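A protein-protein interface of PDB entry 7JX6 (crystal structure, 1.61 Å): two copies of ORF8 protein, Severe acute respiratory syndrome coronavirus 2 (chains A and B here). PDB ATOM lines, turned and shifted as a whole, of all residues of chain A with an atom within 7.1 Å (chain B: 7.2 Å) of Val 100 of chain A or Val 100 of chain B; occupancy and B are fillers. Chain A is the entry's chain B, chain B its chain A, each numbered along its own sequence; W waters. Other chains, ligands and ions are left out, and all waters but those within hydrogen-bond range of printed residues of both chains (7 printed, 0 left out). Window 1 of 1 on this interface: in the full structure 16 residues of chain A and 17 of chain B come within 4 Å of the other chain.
Gln 1 of chain A touches Asp 102 of chain B, but with the chains exchanged Asp 102 of chain A does not touch Gln 1 of chain B (4.9 Å). Cys 3 of chain B touches its own counterpart, Cys 3 of chain A. Cys 3 of chain A touches Leu 5 of chain B, and with the chains exchanged Leu 5 of chain A touches Cys 3 of chain B. Arg 98 of chain A touches Val 100 of chain B, and with the chains exchanged Val 100 of chain A touches Arg 98 of chain B. Of the 22 pairs that touch across the chains among the printed residues, 16 have their exchanged pair printed and touching as well.
Of the printed residues of chain B, Val 100 of chain A touches Cys 3 (3.9 Å), Arg 98 (3.2 Å) and Val 100 (3.7 Å). Printed residues of chain B within 4 Å of Leu 101 of chain A: Arg 98. Printed residues of chain A within 4 Å of Leu 5 of chain B: Gln 1 (3.4 Å), Glu 2 (3.5 Å), Cys 3 (3.7 Å) and Arg 98 (3.9 Å). Val 100 of chain B touches just these residues of chain A: Arg 98 (3.3 Å) and Val 100 (3.7 Å). Of the printed residues of chain A, Leu 101 of chain B touches Arg 98 (2.8 Å). Of the printed residues of chain A, Asp 102 of chain B touches Gln 1 (3.0 Å) and Arg 98 (2.9 Å). The nearest residue of chain B that does not touch Val 100 of chain A is Leu 5 of chain B (6.3 Å).
Hydrophobic or aromatic side chains of chain B within 4 Å of the printed part of chain A: Leu 5 and Val 100. Printed residues of chain A that touch a printed residue of chain B: Gln 1, Glu 2, Cys 3, Leu 5, Gln 6, Ser 7, Arg 98, Val 100, Leu 101 and Asp 102. Hydrophobic or aromatic side chains of chain A that line the printed part of chain B: Leu 5 and Val 100.
Water W2 lies within hydrogen-bond range of the guanidinium group of Arg 98 of chain A (2.4 Å), the side-chain carboxylate of Glu 75 of chain B (2.7 Å) and the backbone carbonyl oxygen of Leu 101 of chain B (2.8 Å). Water W1 lies within hydrogen-bond range of OD2 of Asp 102 of chain A (2.6 Å), OE1 of Gln 1 of chain B (2.9 Å) and OG of Ser 7 of chain A (3.4 Å). Water W5 lies within hydrogen-bond range of the side-chain hydroxyl of Ser 80 of chain B (2.6 Å) and the side-chain carboxylate of Asp 102 of chain A (2.7 Å). Water W3 bridges the backbone carbonyl oxygen (O) of Leu 101 of chain B (2.8 Å) and the guanidinium group (NH1) of Arg 98 of chain A (3.3 Å). Water W6 bridges the backbone carbonyl oxygen (O) of Leu 101 of chain A (2.8 Å) and the guanidinium group (NH2) of Arg 98 of chain B (2.9 Å). Water W4 lies within hydrogen-bond range of N of Ser 7 of chain A (2.9 Å) and NE2 of Gln 1 of chain B (3.3 Å).
The side-chain hydroxyl (OG) of Ser 80 of chain A sits close to the guanidinium group (NE) of Arg 98 of chain A (3.4 Å). O of Gln 6 of chain A lies within hydrogen-bond range of N of Asp 102 of chain A (2.8 Å). The backbone NH (N) of Ser 4 of chain A sits at hydrogen-bond distance from the backbone carbonyl oxygen (O) of Arg 98 of chain A (2.7 Å). The side-chain hydroxyl of Tyr 14 of chain B lies within hydrogen-bond range of the side-chain amide oxygen of Gln 6 of chain B (2.6 Å). The backbone NH (N) of Ser 4 of chain B sits at hydrogen-bond distance from the backbone carbonyl oxygen (O) of Arg 98 of chain B (2.8 Å). The side-chain amide nitrogen (NE2) of Gln 6 of chain A sits at hydrogen-bond distance from the side-chain hydroxyl (OG) of Ser 4 of chain A.
Gln 6 of chain B touches Gln 1 of chain A (C to OE1, 3.998 Å). NE2 of Gln 1 of chain A touches CB of Ser 7 of chain B (3.7 Å). Leu 5 of chain B touches Glu 2 of chain A (CD2 to N, 3.5 Å). Leu 5 of chain A touches Gln 1 of chain B. Cys 3 of chain B touches Leu 5 of chain A (CB to N, 3.8 Å). Gln 1 of chain B touches Gln 6 of chain A. NH2 of Arg 98 of chain A touches CG1 of Val 100 of chain B, at 3.3 Å. Cys 3 of chain B touches Val 100 of chain A. Val 100 of chain A touches Arg 98 of chain B. CG2 of Val 100 of chain A touches CG2 of Val 100 of chain B, at 3.7 Å.
The side-chain sulfur of Cys 3 of chain A forms a disulfide with the side-chain sulfur of Cys 3 of chain B (2.0 Å). The backbone carbonyl oxygen of Leu 5 of chain B sits close to the side-chain amide oxygen of Gln 1 of chain A, 3.4 Å away. The side-chain amide oxygen (OE1) of Gln 1 of chain B sits at hydrogen-bond distance from the side-chain hydroxyl (OG) of Ser 7 of chain A, 2.6 Å away. The backbone NH (N) of Leu 5 of chain B sits at hydrogen-bond distance from the side-chain sulfur (SG) of Cys 3 of chain A, at 3.7 Å. O of Leu 101 of chain A sits at hydrogen-bond distance from NH1 of Arg 98 of chain B, 2.9 Å away. O of Leu 101 of chain B lies within hydrogen-bond range of NH1 of Arg 98 of chain A, 2.8 Å away. OD2 of Asp 102 of chain B is in hydrogen-bond range of NE2 of Gln 1 of chain A (3.0 Å). OD1 of Asp 102 of chain A is in salt-bridge range of NH1 of Arg 98 of chain B. SG of Cys 3 of chain A sits close to N of Ser 4 of chain B, 3.7 Å away. The side-chain carboxylate of Asp 102 of chain B is in salt-bridge range of the guanidinium group of Arg 98 of chain A (2.9 Å).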
ATOM      1  N   GLN A   1     -28.348  21.465 -24.170  1.00  0.00           N
ATOM      2  CA  GLN A   1     -27.231  22.248 -24.697  1.00  0.00           C
ATOM      3  C   GLN A   1     -25.936  21.461 -24.582  1.00  0.00           C
ATOM      4  O   GLN A   1     -25.521  21.098 -23.483  1.00  0.00           O
ATOM      5  CB  GLN A   1     -27.096  23.561 -23.942  1.00  0.00           C
ATOM      6  CG  GLN A   1     -27.836  24.714 -24.553  1.00  0.00           C
ATOM      7  CD  GLN A   1     -27.205  26.033 -24.169  1.00  0.00           C
ATOM      8  OE1 GLN A   1     -26.670  26.187 -23.062  1.00  0.00           O
ATOM      9  NE2 GLN A   1     -27.238  26.991 -25.094  1.00  0.00           N
ATOM     10  N   GLU A   2     -25.300  21.157 -25.700  1.00  0.00           N
ATOM     11  CA  GLU A   2     -24.119  20.319 -25.609  1.00  0.00           C
ATOM     12  C   GLU A   2     -23.125  20.755 -26.665  1.00  0.00           C
ATOM     13  O   GLU A   2     -23.510  21.016 -27.801  1.00  0.00           O
ATOM     14  CB  GLU A   2     -24.473  18.837 -25.790  1.00  0.00           C
ATOM     15  CG  GLU A   2     -23.259  17.908 -25.751  1.00  0.00           C
ATOM     16  CD  GLU A   2     -23.629  16.450 -25.628  1.00  0.00           C
ATOM     17  OE1 GLU A   2     -24.812  16.133 -25.348  1.00  0.00           O
ATOM     18  OE2 GLU A   2     -22.727  15.616 -25.827  1.00  0.00           O
ATOM     19  N   CYS A   3     -21.844  20.746 -26.309  1.00  0.00           N
ATOM     20  CA  CYS A   3     -20.810  20.888 -27.312  1.00  0.00           C
ATOM     21  C   CYS A   3     -19.799  19.762 -27.189  1.00  0.00           C
ATOM     22  O   CYS A   3     -19.635  19.146 -26.129  1.00  0.00           O
ATOM     23  CB  CYS A   3     -20.124  22.278 -27.254  1.00  0.00           C
ATOM     24  SG  CYS A   3     -19.312  22.793 -25.695  1.00  0.00           S
ATOM     25  N   SER A   4     -19.169  19.488 -28.316  1.00  0.00           N
ATOM     26  CA  SER A   4     -18.158  18.463 -28.491  1.00  0.00           C
ATOM     27  C   SER A   4     -16.874  19.176 -28.870  1.00  0.00           C
ATOM     28  O   SER A   4     -16.830  19.859 -29.893  1.00  0.00           O
ATOM     29  CB  SER A   4     -18.553  17.465 -29.587  1.00  0.00           C
ATOM     30  OG  SER A   4     -17.478  16.590 -29.876  1.00  0.00           O
ATOM     31  N   LEU A   5     -15.845  19.022 -28.051  1.00  0.00           N
ATOM     32  CA  LEU A   5     -14.535  19.590 -28.332  1.00  0.00           C
ATOM     33  C   LEU A   5     -13.662  18.582 -29.067  1.00  0.00           C
ATOM     34  O   LEU A   5     -13.503  17.449 -28.626  1.00  0.00           O
ATOM     35  CB  LEU A   5     -13.860  19.986 -27.019  1.00  0.00           C
ATOM     36  CG  LEU A   5     -12.457  20.525 -27.233  1.00  0.00           C
ATOM     37  CD1 LEU A   5     -12.520  21.806 -28.069  1.00  0.00           C
ATOM     38  CD2 LEU A   5     -11.850  20.850 -25.877  1.00  0.00           C
ATOM     39  N   GLN A   6     -13.093  18.991 -30.190  1.00  0.00           N
ATOM     40  CA  GLN A   6     -12.244  18.091 -30.966  1.00  0.00           C
ATOM     41  C   GLN A   6     -11.018  18.873 -31.394  1.00  0.00           C
ATOM     42  O   GLN A   6     -11.052  20.100 -31.415  1.00  0.00           O
ATOM     43  CB  GLN A   6     -13.016  17.527 -32.181  1.00  0.00           C
ATOM     44  CG  GLN A   6     -14.337  16.872 -31.733  1.00  0.00           C
ATOM     45  CD  GLN A   6     -14.985  15.963 -32.777  1.00  0.00           C
ATOM     46  OE1 GLN A   6     -14.351  15.534 -33.740  1.00  0.00           O
ATOM     47  NE2 GLN A   6     -16.263  15.669 -32.577  1.00  0.00           N
ATOM     48  N   SER A   7      -9.947  18.167 -31.775  1.00  0.00           N
ATOM     49  CA  SER A   7      -8.691  18.817 -32.158  1.00  0.00           C
ATOM     50  C   SER A   7      -8.239  18.377 -33.547  1.00  0.00           C
ATOM     51  O   SER A   7      -8.391  17.207 -33.924  1.00  0.00           O
ATOM     52  CB  SER A   7      -7.565  18.516 -31.153  1.00  0.00           C
ATOM     53  OG  SER A   7      -7.823  19.133 -29.919  1.00  0.00           O
ATOM     54  N   GLU A  75     -12.999  26.836 -38.268  1.00  0.00           N
ATOM     55  CA  GLU A  75     -14.333  27.278 -37.909  1.00  0.00           C
ATOM     56  C   GLU A  75     -14.994  27.875 -39.143  1.00  0.00           C
ATOM     57  O   GLU A  75     -14.402  28.738 -39.794  1.00  0.00           O
ATOM     58  CB  GLU A  75     -14.265  28.305 -36.780  1.00  0.00           C
ATOM     59  CG  GLU A  75     -15.593  28.777 -36.264  1.00  0.00           C
ATOM     60  CD  GLU A  75     -16.360  27.681 -35.535  1.00  0.00           C
ATOM     61  OE1 GLU A  75     -15.808  26.570 -35.365  1.00  0.00           O
ATOM     62  OE2 GLU A  75     -17.507  27.942 -35.126  1.00  0.00           O
ATOM     63  N   SER A  80     -21.084  27.755 -36.407  1.00  0.00           N
ATOM     64  CA  SER A  80     -20.497  26.513 -35.920  1.00  0.00           C
ATOM     65  C   SER A  80     -21.003  25.312 -36.698  1.00  0.00           C
ATOM     66  O   SER A  80     -22.120  25.320 -37.234  1.00  0.00           O
ATOM     67  CB  SER A  80     -20.839  26.319 -34.450  1.00  0.00           C
ATOM     68  OG  SER A  80     -22.187  26.709 -34.231  1.00  0.00           O
ATOM     69  N   LEU A  81     -20.132  24.302 -36.808  1.00  0.00           N
ATOM     70  CA  LEU A  81     -20.573  22.965 -37.161  1.00  0.00           C
ATOM     71  C   LEU A  81     -21.506  22.471 -36.062  1.00  0.00           C
ATOM     72  O   LEU A  81     -21.242  22.665 -34.866  1.00  0.00           O
ATOM     73  CB  LEU A  81     -19.373  22.036 -37.342  1.00  0.00           C
ATOM     74  CG  LEU A  81     -19.634  20.555 -37.678  1.00  0.00           C
ATOM     75  CD1 LEU A  81     -20.357  20.462 -39.020  1.00  0.00           C
ATOM     76  CD2 LEU A  81     -18.364  19.744 -37.691  1.00  0.00           C
ATOM     77  N   VAL A  97     -25.636  18.931 -31.197  1.00  0.00           N
ATOM     78  CA  VAL A  97     -24.358  19.116 -30.517  1.00  0.00           C
ATOM     79  C   VAL A  97     -23.521  20.051 -31.372  1.00  0.00           C
ATOM     80  O   VAL A  97     -23.280  19.774 -32.554  1.00  0.00           O
ATOM     81  CB  VAL A  97     -23.643  17.774 -30.313  1.00  0.00           C
ATOM     82  CG1 VAL A  97     -22.310  17.993 -29.631  1.00  0.00           C
ATOM     83  CG2 VAL A  97     -24.524  16.808 -29.497  1.00  0.00           C
ATOM     84  N   ARG A  98     -23.043  21.140 -30.768  1.00  0.00           N
ATOM     85  CA  ARG A  98     -22.128  22.037 -31.454  1.00  0.00           C
ATOM     86  C   ARG A  98     -20.727  21.433 -31.401  1.00  0.00           C
ATOM     87  O   ARG A  98     -20.294  20.968 -30.338  1.00  0.00           O
ATOM     88  CB  ARG A  98     -22.177  23.401 -30.769  1.00  0.00           C
ATOM     89  CG  ARG A  98     -21.332  24.459 -31.397  1.00  0.00           C
ATOM     90  CD  ARG A  98     -21.767  25.822 -30.854  1.00  0.00           C
ATOM     91  NE  ARG A  98     -20.784  26.834 -31.144  1.00  0.00           N
ATOM     92  CZ  ARG A  98     -20.761  27.994 -30.527  1.00  0.00           C
ATOM     93  NH1 ARG A  98     -21.667  28.248 -29.589  1.00  0.00           N
ATOM     94  NH2 ARG A  98     -19.822  28.876 -30.813  1.00  0.00           N
ATOM     95  N   VAL A  99     -20.033  21.391 -32.537  1.00  0.00           N
ATOM     96  CA  VAL A  99     -18.656  20.910 -32.576  1.00  0.00           C
ATOM     97  C   VAL A  99     -17.748  22.123 -32.567  1.00  0.00           C
ATOM     98  O   VAL A  99     -17.930  23.075 -33.352  1.00  0.00           O
ATOM     99  CB  VAL A  99     -18.351  20.012 -33.786  1.00  0.00           C
ATOM    100  CG1 VAL A  99     -16.871  19.606 -33.762  1.00  0.00           C
ATOM    101  CG2 VAL A  99     -19.218  18.735 -33.782  1.00  0.00           C
ATOM    102  N   VAL A 100     -16.780  22.077 -31.658  1.00  0.00           N
ATOM    103  CA  VAL A 100     -15.866  23.164 -31.324  1.00  0.00           C
ATOM    104  C   VAL A 100     -14.458  22.640 -31.573  1.00  0.00           C
ATOM    105  O   VAL A 100     -14.133  21.536 -31.128  1.00  0.00           O
ATOM    106  CB  VAL A 100     -16.058  23.520 -29.834  1.00  0.00           C
ATOM    107  CG1 VAL A 100     -15.087  24.521 -29.360  1.00  0.00           C
ATOM    108  CG2 VAL A 100     -17.490  23.971 -29.567  1.00  0.00           C
ATOM    109  N   LEU A 101     -13.610  23.405 -32.262  1.00  0.00           N
ATOM    110  CA  LEU A 101     -12.298  22.897 -32.645  1.00  0.00           C
ATOM    111  C   LEU A 101     -11.183  23.578 -31.870  1.00  0.00           C
ATOM    112  O   LEU A 101     -11.085  24.815 -31.868  1.00  0.00           O
ATOM    113  CB  LEU A 101     -12.041  23.095 -34.138  1.00  0.00           C
ATOM    114  CG  LEU A 101     -13.061  22.372 -35.023  1.00  0.00           C
ATOM    115  CD1 LEU A 101     -12.656  22.651 -36.473  1.00  0.00           C
ATOM    116  CD2 LEU A 101     -13.069  20.861 -34.775  1.00  0.00           C
ATOM    117  N   ASP A 102     -10.328  22.775 -31.242  1.00  0.00           N
ATOM    118  CA  ASP A 102      -9.004  23.258 -30.864  1.00  0.00           C
ATOM    119  C   ASP A 102      -8.023  22.940 -31.984  1.00  0.00           C
ATOM    120  O   ASP A 102      -8.037  21.846 -32.548  1.00  0.00           O
ATOM    121  CB  ASP A 102      -8.520  22.601 -29.581  1.00  0.00           C
ATOM    122  CG  ASP A 102      -9.075  23.238 -28.330  1.00  0.00           C
ATOM    123  OD1 ASP A 102      -9.710  24.325 -28.376  1.00  0.00           O
ATOM    124  OD2 ASP A 102      -8.854  22.611 -27.256  1.00  0.00           O
ATOM    125  N   GLN B   1     -10.928  15.716 -23.677  1.00  0.00           N
ATOM    126  CA  GLN B   1     -11.282  17.060 -24.082  1.00  0.00           C
ATOM    127  C   GLN B   1     -12.708  17.317 -23.694  1.00  0.00           C
ATOM    128  O   GLN B   1     -13.604  16.728 -24.285  1.00  0.00           O
ATOM    129  CB  GLN B   1     -11.142  17.236 -25.592  1.00  0.00           C
ATOM    130  CG  GLN B   1      -9.758  17.050 -26.134  1.00  0.00           C
ATOM    131  CD  GLN B   1      -9.794  16.933 -27.628  1.00  0.00           C
ATOM    132  OE1 GLN B   1      -9.453  17.864 -28.329  1.00  0.00           O
ATOM    133  NE2 GLN B   1     -10.256  15.797 -28.126  1.00  0.00           N
ATOM    134  N   CYS B   3     -16.025  20.137 -22.886  1.00  0.00           N
ATOM    135  CA  CYS B   3     -16.604  21.320 -23.512  1.00  0.00           C
ATOM    136  C   CYS B   3     -17.845  21.694 -22.725  1.00  0.00           C
ATOM    137  O   CYS B   3     -18.746  20.857 -22.579  1.00  0.00           O
ATOM    138  CB  CYS B   3     -16.996  20.980 -24.967  1.00  0.00           C
ATOM    139  SG  CYS B   3     -17.335  22.463 -25.937  1.00  0.00           S
ATOM    140  N   SER B   4     -17.913  22.933 -22.257  1.00  0.00           N
ATOM    141  CA  SER B   4     -19.058  23.489 -21.555  1.00  0.00           C
ATOM    142  C   SER B   4     -19.739  24.500 -22.459  1.00  0.00           C
ATOM    143  O   SER B   4     -19.097  25.460 -22.883  1.00  0.00           O
ATOM    144  CB  SER B   4     -18.602  24.157 -20.270  1.00  0.00           C
ATOM    145  OG  SER B   4     -19.682  24.847 -19.676  1.00  0.00           O
ATOM    146  N   LEU B   5     -21.016  24.261 -22.781  1.00  0.00           N
ATOM    147  CA  LEU B   5     -21.789  25.151 -23.633  1.00  0.00           C
ATOM    148  C   LEU B   5     -22.715  25.956 -22.738  1.00  0.00           C
ATOM    149  O   LEU B   5     -23.541  25.379 -22.030  1.00  0.00           O
ATOM    150  CB  LEU B   5     -22.600  24.369 -24.665  1.00  0.00           C
ATOM    151  CG  LEU B   5     -23.378  25.237 -25.647  1.00  0.00           C
ATOM    152  CD1 LEU B   5     -22.480  26.183 -26.428  1.00  0.00           C
ATOM    153  CD2 LEU B   5     -24.094  24.311 -26.603  1.00  0.00           C
ATOM    154  N   GLN B   6     -22.534  27.274 -22.724  1.00  0.00           N
ATOM    155  CA  GLN B   6     -23.333  28.154 -21.887  1.00  0.00           C
ATOM    156  C   GLN B   6     -24.040  29.183 -22.759  1.00  0.00           C
ATOM    157  O   GLN B   6     -23.690  29.381 -23.913  1.00  0.00           O
ATOM    158  CB  GLN B   6     -22.463  28.833 -20.827  1.00  0.00           C
ATOM    159  CG  GLN B   6     -21.766  27.794 -19.927  1.00  0.00           C
ATOM    160  CD  GLN B   6     -21.010  28.385 -18.755  1.00  0.00           C
ATOM    161  OE1 GLN B   6     -21.335  29.465 -18.262  1.00  0.00           O
ATOM    162  NE2 GLN B   6     -19.993  27.660 -18.283  1.00  0.00           N
ATOM    163  N   SER B   7     -25.058  29.829 -22.209  1.00  0.00           N
ATOM    164  CA  SER B   7     -25.802  30.803 -22.992  1.00  0.00           C
ATOM    165  C   SER B   7     -25.888  32.117 -22.232  1.00  0.00           C
ATOM    166  O   SER B   7     -25.996  32.131 -21.001  1.00  0.00           O
ATOM    167  CB  SER B   7     -27.206  30.272 -23.344  1.00  0.00           C
ATOM    168  OG  SER B   7     -27.882  29.820 -22.191  1.00  0.00           O
ATOM    169  N   TYR B  14     -21.995  38.584 -17.889  1.00  0.00           N
ATOM    170  CA  TYR B  14     -22.406  37.208 -17.650  1.00  0.00           C
ATOM    171  C   TYR B  14     -21.454  36.608 -16.637  1.00  0.00           C
ATOM    172  O   TYR B  14     -20.250  36.548 -16.898  1.00  0.00           O
ATOM    173  CB  TYR B  14     -22.386  36.415 -18.953  1.00  0.00           C
ATOM    174  CG  TYR B  14     -22.671  34.961 -18.803  1.00  0.00           C
ATOM    175  CD1 TYR B  14     -23.872  34.514 -18.229  1.00  0.00           C
ATOM    176  CD2 TYR B  14     -21.735  34.015 -19.186  1.00  0.00           C
ATOM    177  CE1 TYR B  14     -24.147  33.178 -18.076  1.00  0.00           C
ATOM    178  CE2 TYR B  14     -22.002  32.666 -19.025  1.00  0.00           C
ATOM    179  CZ  TYR B  14     -23.201  32.252 -18.473  1.00  0.00           C
ATOM    180  OH  TYR B  14     -23.461  30.898 -18.328  1.00  0.00           O
ATOM    181  N   ALA B  34      -7.276  29.811 -30.239  1.00  0.00           N
ATOM    182  CA  ALA B  34      -7.743  28.450 -29.905  1.00  0.00           C
ATOM    183  C   ALA B  34      -6.750  27.389 -30.379  1.00  0.00           C
ATOM    184  O   ALA B  34      -7.110  26.249 -30.658  1.00  0.00           O
ATOM    185  CB  ALA B  34      -9.151  28.190 -30.472  1.00  0.00           C
ATOM    186  N   GLU B  75     -17.751  35.900 -27.625  1.00  0.00           N
ATOM    187  CA  GLU B  75     -16.580  35.061 -27.831  1.00  0.00           C
ATOM    188  C   GLU B  75     -15.358  35.960 -27.876  1.00  0.00           C
ATOM    189  O   GLU B  75     -15.379  36.983 -28.567  1.00  0.00           O
ATOM    190  CB  GLU B  75     -16.680  34.254 -29.119  1.00  0.00           C
ATOM    191  CG  GLU B  75     -17.654  33.108 -29.023  1.00  0.00           C
ATOM    192  CD  GLU B  75     -17.163  31.967 -28.118  1.00  0.00           C
ATOM    193  OE1 GLU B  75     -15.964  31.913 -27.773  1.00  0.00           O
ATOM    194  OE2 GLU B  75     -17.984  31.120 -27.755  1.00  0.00           O
ATOM    195  N   SER B  80      -9.768  31.164 -27.488  1.00  0.00           N
ATOM    196  CA  SER B  80     -10.775  30.371 -26.795  1.00  0.00           C
ATOM    197  C   SER B  80     -10.734  30.653 -25.303  1.00  0.00           C
ATOM    198  O   SER B  80      -9.688  30.972 -24.752  1.00  0.00           O
ATOM    199  CB  SER B  80     -10.514  28.899 -27.056  1.00  0.00           C
ATOM    200  OG  SER B  80      -9.181  28.522 -26.721  1.00  0.00           O
ATOM    201  N   LEU B  81     -11.876  30.494 -24.640  1.00  0.00           N
ATOM    202  CA  LEU B  81     -11.934  30.608 -23.184  1.00  0.00           C
ATOM    203  C   LEU B  81     -11.746  29.226 -22.575  1.00  0.00           C
ATOM    204  O   LEU B  81     -12.505  28.310 -22.909  1.00  0.00           O
ATOM    205  CB  LEU B  81     -13.270  31.192 -22.750  1.00  0.00           C
ATOM    206  CG  LEU B  81     -13.485  31.319 -21.255  1.00  0.00           C
ATOM    207  CD1 LEU B  81     -12.460  32.293 -20.675  1.00  0.00           C
ATOM    208  CD2 LEU B  81     -14.911  31.779 -20.938  1.00  0.00           C
ATOM    209  N   VAL B  97     -11.326  22.624 -19.347  1.00  0.00           N
ATOM    210  CA  VAL B  97     -12.644  22.666 -19.958  1.00  0.00           C
ATOM    211  C   VAL B  97     -12.706  23.905 -20.822  1.00  0.00           C
ATOM    212  O   VAL B  97     -12.449  25.009 -20.334  1.00  0.00           O
ATOM    213  CB  VAL B  97     -13.765  22.716 -18.925  1.00  0.00           C
ATOM    214  CG1 VAL B  97     -15.092  22.619 -19.658  1.00  0.00           C
ATOM    215  CG2 VAL B  97     -13.597  21.541 -17.921  1.00  0.00           C
ATOM    216  N   ARG B  98     -13.054  23.730 -22.089  1.00  0.00           N
ATOM    217  CA  ARG B  98     -13.309  24.885 -22.935  1.00  0.00           C
ATOM    218  C   ARG B  98     -14.741  25.356 -22.735  1.00  0.00           C
ATOM    219  O   ARG B  98     -15.659  24.543 -22.663  1.00  0.00           O
ATOM    220  CB  ARG B  98     -13.095  24.536 -24.405  1.00  0.00           C
ATOM    221  CG  ARG B  98     -13.289  25.769 -25.268  1.00  0.00           C
ATOM    222  CD  ARG B  98     -12.683  25.572 -26.620  1.00  0.00           C
ATOM    223  NE  ARG B  98     -13.098  26.641 -27.530  1.00  0.00           N
ATOM    224  CZ  ARG B  98     -12.739  26.657 -28.801  1.00  0.00           C
ATOM    225  NH1 ARG B  98     -11.983  25.684 -29.280  1.00  0.00           N
ATOM    226  NH2 ARG B  98     -13.171  27.631 -29.600  1.00  0.00           N
ATOM    227  N   VAL B  99     -14.945  26.672 -22.689  1.00  0.00           N
ATOM    228  CA  VAL B  99     -16.274  27.234 -22.515  1.00  0.00           C
ATOM    229  C   VAL B  99     -16.654  27.944 -23.799  1.00  0.00           C
ATOM    230  O   VAL B  99     -15.912  28.806 -24.274  1.00  0.00           O
ATOM    231  CB  VAL B  99     -16.348  28.202 -21.328  1.00  0.00           C
ATOM    232  CG1 VAL B  99     -17.721  28.821 -21.271  1.00  0.00           C
ATOM    233  CG2 VAL B  99     -16.071  27.463 -20.052  1.00  0.00           C
ATOM    234  N   VAL B 100     -17.812  27.583 -24.342  1.00  0.00           N
ATOM    235  CA  VAL B 100     -18.303  28.136 -25.598  1.00  0.00           C
ATOM    236  C   VAL B 100     -19.667  28.734 -25.306  1.00  0.00           C
ATOM    237  O   VAL B 100     -20.363  28.259 -24.413  1.00  0.00           O
ATOM    238  CB  VAL B 100     -18.412  27.026 -26.662  1.00  0.00           C
ATOM    239  CG1 VAL B 100     -18.610  27.646 -27.986  1.00  0.00           C
ATOM    240  CG2 VAL B 100     -17.146  26.144 -26.640  1.00  0.00           C
ATOM    241  N   LEU B 101     -20.039  29.792 -26.032  1.00  0.00           N
ATOM    242  CA  LEU B 101     -21.273  30.520 -25.752  1.00  0.00           C
ATOM    243  C   LEU B 101     -22.214  30.457 -26.946  1.00  0.00           C
ATOM    244  O   LEU B 101     -21.789  30.662 -28.083  1.00  0.00           O
ATOM    245  CB  LEU B 101     -20.996  31.989 -25.396  1.00  0.00           C
ATOM    246  CG  LEU B 101     -19.965  32.307 -24.304  1.00  0.00           C
ATOM    247  CD1 LEU B 101     -19.818  33.828 -24.152  1.00  0.00           C
ATOM    248  CD2 LEU B 101     -20.403  31.690 -22.981  1.00  0.00           C
ATOM    249  N   ASP B 102     -23.471  30.102 -26.683  1.00  0.00           N
ATOM    250  CA  ASP B 102     -24.615  30.445 -27.535  1.00  0.00           C
ATOM    251  C   ASP B 102     -25.201  31.780 -27.077  1.00  0.00           C
ATOM    252  O   ASP B 102     -25.325  32.035 -25.880  1.00  0.00           O
ATOM    253  CB  ASP B 102     -25.710  29.378 -27.442  1.00  0.00           C
ATOM    254  CG  ASP B 102     -25.370  28.101 -28.182  1.00  0.00           C
ATOM    255  OD1 ASP B 102     -24.472  28.088 -29.046  1.00  0.00           O
ATOM    256  OD2 ASP B 102     -26.030  27.084 -27.889  1.00  0.00           O
HETATM  257  O   HOH W   1      -8.398  20.110 -26.740  1.00  0.00           O
HETATM  258  O   HOH W   2     -19.648  31.080 -29.818  1.00  0.00           O
HETATM  259  O   HOH W   3     -22.576  31.221 -30.686  1.00  0.00           O
HETATM  260  O   HOH W   4     -10.093  15.309 -31.392  1.00  0.00           O
HETATM  261  O   HOH W   5      -8.818  25.944 -26.459  1.00  0.00           O
HETATM  262  O   HOH W   6     -12.296  27.320 -32.371  1.00  0.00           O
HETATM  263  O   HOH W   7     -23.835  28.979 -32.228  1.00  0.00           O
